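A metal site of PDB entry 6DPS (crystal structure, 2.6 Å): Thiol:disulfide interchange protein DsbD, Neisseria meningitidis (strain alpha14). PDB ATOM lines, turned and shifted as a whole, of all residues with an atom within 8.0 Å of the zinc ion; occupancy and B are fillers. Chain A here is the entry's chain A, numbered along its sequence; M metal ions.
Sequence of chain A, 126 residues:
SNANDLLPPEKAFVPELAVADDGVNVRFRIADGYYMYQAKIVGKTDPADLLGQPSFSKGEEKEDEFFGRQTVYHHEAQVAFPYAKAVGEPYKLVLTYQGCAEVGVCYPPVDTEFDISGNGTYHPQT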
ATOM      1  N   GLY A  33     -30.491 -19.544   8.728  1.00  0.00           N
ATOM      2  CA  GLY A  33     -29.122 -19.056   8.798  1.00  0.00           C
ATOM      3  C   GLY A  33     -28.310 -19.579   9.974  1.00  0.00           C
ATOM      4  O   GLY A  33     -27.184 -19.092  10.190  1.00  0.00           O
ATOM      5  N   TYR A  34     -28.846 -20.538  10.738  1.00  0.00           N
ATOM      6  CA  TYR A  34     -28.147 -21.135  11.876  1.00  0.00           C
ATOM      7  C   TYR A  34     -28.207 -22.646  11.741  1.00  0.00           C
ATOM      8  O   TYR A  34     -28.970 -23.167  10.932  1.00  0.00           O
ATOM      9  CB  TYR A  34     -28.762 -20.649  13.210  1.00  0.00           C
ATOM     10  CG  TYR A  34     -28.666 -19.154  13.357  1.00  0.00           C
ATOM     11  CD1 TYR A  34     -29.562 -18.315  12.703  1.00  0.00           C
ATOM     12  CD2 TYR A  34     -27.640 -18.562  14.116  1.00  0.00           C
ATOM     13  CE1 TYR A  34     -29.453 -16.945  12.806  1.00  0.00           C
ATOM     14  CE2 TYR A  34     -27.533 -17.182  14.222  1.00  0.00           C
ATOM     15  CZ  TYR A  34     -28.454 -16.371  13.564  1.00  0.00           C
ATOM     16  OH  TYR A  34     -28.387 -14.996  13.654  1.00  0.00           O
ATOM     17  N   TYR A  35     -27.370 -23.346  12.512  1.00  0.00           N
ATOM     18  CA  TYR A  35     -27.390 -24.810  12.526  1.00  0.00           C
ATOM     19  C   TYR A  35     -26.834 -25.313  13.838  1.00  0.00           C
ATOM     20  O   TYR A  35     -26.273 -24.543  14.621  1.00  0.00           O
ATOM     21  CB  TYR A  35     -26.571 -25.418  11.383  1.00  0.00           C
ATOM     22  CG  TYR A  35     -25.114 -25.096  11.406  1.00  0.00           C
ATOM     23  CD1 TYR A  35     -24.631 -23.929  10.817  1.00  0.00           C
ATOM     24  CD2 TYR A  35     -24.203 -25.983  11.962  1.00  0.00           C
ATOM     25  CE1 TYR A  35     -23.282 -23.644  10.795  1.00  0.00           C
ATOM     26  CE2 TYR A  35     -22.833 -25.707  11.951  1.00  0.00           C
ATOM     27  CZ  TYR A  35     -22.390 -24.530  11.361  1.00  0.00           C
ATOM     28  OH  TYR A  35     -21.054 -24.223  11.329  1.00  0.00           O
ATOM     29  N   MET A  36     -27.012 -26.613  14.094  1.00  0.00           N
ATOM     30  CA  MET A  36     -26.693 -27.202  15.393  1.00  0.00           C
ATOM     31  C   MET A  36     -25.865 -28.471  15.234  1.00  0.00           C
ATOM     32  O   MET A  36     -26.057 -29.244  14.297  1.00  0.00           O
ATOM     33  CB  MET A  36     -27.963 -27.538  16.198  1.00  0.00           C
ATOM     34  CG  MET A  36     -28.723 -26.346  16.774  1.00  0.00           C
ATOM     35  SD  MET A  36     -30.207 -26.925  17.624  1.00  0.00           S
ATOM     36  CE  MET A  36     -29.498 -27.220  19.245  1.00  0.00           C
ATOM     37  N   GLU A  60     -27.921 -33.701   8.639  1.00  0.00           N
ATOM     38  CA  GLU A  60     -27.036 -33.668   7.486  1.00  0.00           C
ATOM     39  C   GLU A  60     -25.564 -33.602   7.892  1.00  0.00           C
ATOM     40  O   GLU A  60     -25.213 -33.250   9.024  1.00  0.00           O
ATOM     41  CB  GLU A  60     -27.319 -32.488   6.559  1.00  0.00           C
ATOM     42  CG  GLU A  60     -28.746 -32.404   6.139  1.00  0.00           C
ATOM     43  CD  GLU A  60     -29.484 -31.404   6.960  1.00  0.00           C
ATOM     44  OE1 GLU A  60     -30.527 -31.749   7.544  1.00  0.00           O
ATOM     45  OE2 GLU A  60     -28.990 -30.275   7.032  1.00  0.00           O
ATOM     46  N   GLU A  61     -24.727 -33.926   6.926  1.00  0.00           N
ATOM     47  CA  GLU A  61     -23.295 -33.979   7.110  1.00  0.00           C
ATOM     48  C   GLU A  61     -22.707 -32.681   6.576  1.00  0.00           C
ATOM     49  O   GLU A  61     -23.172 -32.151   5.567  1.00  0.00           O
ATOM     50  CB  GLU A  61     -22.709 -35.187   6.379  1.00  0.00           C
ATOM     51  CG  GLU A  61     -21.224 -35.367   6.531  1.00  0.00           C
ATOM     52  CD  GLU A  61     -20.776 -36.695   5.959  1.00  0.00           C
ATOM     53  OE1 GLU A  61     -20.111 -36.683   4.902  1.00  0.00           O
ATOM     54  OE2 GLU A  61     -21.098 -37.733   6.563  1.00  0.00           O
ATOM     55  N   LYS A  62     -21.742 -32.147   7.296  1.00  0.00           N
ATOM     56  CA  LYS A  62     -21.181 -30.872   6.896  1.00  0.00           C
ATOM     57  C   LYS A  62     -19.707 -30.863   7.220  1.00  0.00           C
ATOM     58  O   LYS A  62     -19.286 -31.348   8.284  1.00  0.00           O
ATOM     59  CB  LYS A  62     -21.878 -29.691   7.586  1.00  0.00           C
ATOM     60  CG  LYS A  62     -21.057 -28.419   7.613  1.00  0.00           C
ATOM     61  CD  LYS A  62     -21.711 -27.340   8.465  1.00  0.00           C
ATOM     62  CE  LYS A  62     -23.084 -27.003   7.878  1.00  0.00           C
ATOM     63  NZ  LYS A  62     -23.657 -25.714   8.334  1.00  0.00           N
ATOM     64  N   GLU A  63     -18.928 -30.332   6.308  1.00  0.00           N
ATOM     65  CA  GLU A  63     -17.537 -30.006   6.571  1.00  0.00           C
ATOM     66  C   GLU A  63     -17.508 -28.625   7.221  1.00  0.00           C
ATOM     67  O   GLU A  63     -17.890 -27.619   6.603  1.00  0.00           O
ATOM     68  CB  GLU A  63     -16.697 -30.049   5.287  1.00  0.00           C
ATOM     69  CG  GLU A  63     -15.318 -29.393   5.388  1.00  0.00           C
ATOM     70  CD  GLU A  63     -14.455 -29.752   6.608  1.00  0.00           C
ATOM     71  OE1 GLU A  63     -14.714 -30.794   7.304  1.00  0.00           O
ATOM     72  OE2 GLU A  63     -13.474 -29.010   6.827  1.00  0.00           O
ATOM     73  N   ASP A  64     -17.127 -28.580   8.465  1.00  0.00           N
ATOM     74  CA  ASP A  64     -17.241 -27.425   9.321  1.00  0.00           C
ATOM     75  C   ASP A  64     -15.857 -26.891   9.644  1.00  0.00           C
ATOM     76  O   ASP A  64     -14.902 -27.634   9.865  1.00  0.00           O
ATOM     77  CB  ASP A  64     -18.027 -27.805  10.600  1.00  0.00           C
ATOM     78  CG  ASP A  64     -18.217 -26.660  11.516  1.00  0.00           C
ATOM     79  OD1 ASP A  64     -17.344 -26.469  12.380  1.00  0.00           O
ATOM     80  OD2 ASP A  64     -19.258 -25.975  11.417  1.00  0.00           O
ATOM     81  N   VAL A  72     -25.044 -32.225  11.377  1.00  0.00           N
ATOM     82  CA  VAL A  72     -25.605 -30.972  11.853  1.00  0.00           C
ATOM     83  C   VAL A  72     -27.099 -30.939  11.582  1.00  0.00           C
ATOM     84  O   VAL A  72     -27.654 -31.825  10.943  1.00  0.00           O
ATOM     85  CB  VAL A  72     -24.918 -29.729  11.245  1.00  0.00           C
ATOM     86  CG1 VAL A  72     -23.454 -29.739  11.581  1.00  0.00           C
ATOM     87  CG2 VAL A  72     -25.103 -29.691   9.746  1.00  0.00           C
ATOM     88  N   TYR A  73     -27.733 -29.886  12.064  1.00  0.00           N
ATOM     89  CA  TYR A  73     -29.174 -29.702  11.936  1.00  0.00           C
ATOM     90  C   TYR A  73     -29.494 -28.293  11.443  1.00  0.00           C
ATOM     91  O   TYR A  73     -29.161 -27.303  12.104  1.00  0.00           O
ATOM     92  CB  TYR A  73     -29.878 -29.947  13.272  1.00  0.00           C
ATOM     93  CG  TYR A  73     -29.925 -31.382  13.729  1.00  0.00           C
ATOM     94  CD1 TYR A  73     -30.705 -32.320  13.056  1.00  0.00           C
ATOM     95  CD2 TYR A  73     -29.210 -31.799  14.841  1.00  0.00           C
ATOM     96  CE1 TYR A  73     -30.749 -33.632  13.482  1.00  0.00           C
ATOM     97  CE2 TYR A  73     -29.258 -33.093  15.272  1.00  0.00           C
ATOM     98  CZ  TYR A  73     -30.024 -34.015  14.596  1.00  0.00           C
ATOM     99  OH  TYR A  73     -30.057 -35.316  15.029  1.00  0.00           O
ATOM    100  N   HIS A  74     -30.147 -28.209  10.297  1.00  0.00           N
ATOM    101  CA  HIS A  74     -30.839 -27.008   9.869  1.00  0.00           C
ATOM    102  C   HIS A  74     -32.345 -27.145  10.150  1.00  0.00           C
ATOM    103  O   HIS A  74     -32.905 -28.242  10.120  1.00  0.00           O
ATOM    104  CB  HIS A  74     -30.599 -26.754   8.384  1.00  0.00           C
ATOM    105  CG  HIS A  74     -29.157 -26.683   7.994  1.00  0.00           C
ATOM    106  ND1 HIS A  74     -28.483 -27.734   7.412  1.00  0.00           N
ATOM    107  CD2 HIS A  74     -28.255 -25.680   8.127  1.00  0.00           C
ATOM    108  CE1 HIS A  74     -27.224 -27.380   7.189  1.00  0.00           C
ATOM    109  NE2 HIS A  74     -27.066 -26.134   7.617  1.00  0.00           N
ATOM    110  N   CYS A 100     -24.432 -22.717  15.630  1.00  0.00           N
ATOM    111  CA  CYS A 100     -23.592 -21.742  14.942  1.00  0.00           C
ATOM    112  C   CYS A 100     -24.422 -20.949  13.948  1.00  0.00           C
ATOM    113  O   CYS A 100     -25.563 -21.315  13.628  1.00  0.00           O
ATOM    114  CB  CYS A 100     -22.414 -22.423  14.194  1.00  0.00           C
ATOM    115  SG  CYS A 100     -21.333 -23.472  15.211  1.00  0.00           S
ATOM    116  N   ALA A 101     -23.821 -19.882  13.425  1.00  0.00           N
ATOM    117  CA  ALA A 101     -24.399 -19.123  12.330  1.00  0.00           C
ATOM    118  C   ALA A 101     -23.685 -19.483  11.030  1.00  0.00           C
ATOM    119  O   ALA A 101     -22.462 -19.622  11.015  1.00  0.00           O
ATOM    120  CB  ALA A 101     -24.318 -17.626  12.611  1.00  0.00           C
ATOM    121  N   GLU A 102     -24.448 -19.619   9.950  1.00  0.00           N
ATOM    122  CA  GLU A 102     -23.881 -19.903   8.627  1.00  0.00           C
ATOM    123  C   GLU A 102     -22.889 -18.845   8.166  1.00  0.00           C
ATOM    124  O   GLU A 102     -22.035 -19.143   7.323  1.00  0.00           O
ATOM    125  CB  GLU A 102     -25.009 -20.009   7.602  1.00  0.00           C
ATOM    126  CG  GLU A 102     -26.018 -21.093   7.940  1.00  0.00           C
ATOM    127  CD  GLU A 102     -25.549 -22.496   7.593  1.00  0.00           C
ATOM    128  OE1 GLU A 102     -24.387 -22.678   7.189  1.00  0.00           O
ATOM    129  OE2 GLU A 102     -26.366 -23.416   7.720  1.00  0.00           O
HETATM  130 ZN    ZN M   1     -25.399 -25.252   7.048  1.00  0.00          ZN
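Within 4 Å of the zinc ion: Lys 62, His 74 and Glu 102.
ND1 of His 74 sits at hydrogen-bond distance from OE2 of Glu 60 (2.6 Å). The backbone NH (N) of Glu 102 lies within hydrogen-bond range of the backbone carbonyl oxygen (O) of Gly 33 (2.8 Å).
NE2 of His 74 is bound to the zinc ion. The zinc ion is bound by OE2 of Glu 102 (2.2 Å). NZ of Lys 62 binds the zinc ion (2.2 Å). Slightly farther from the zinc ion lies OE1 of Glu 102 (2.8 Å).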
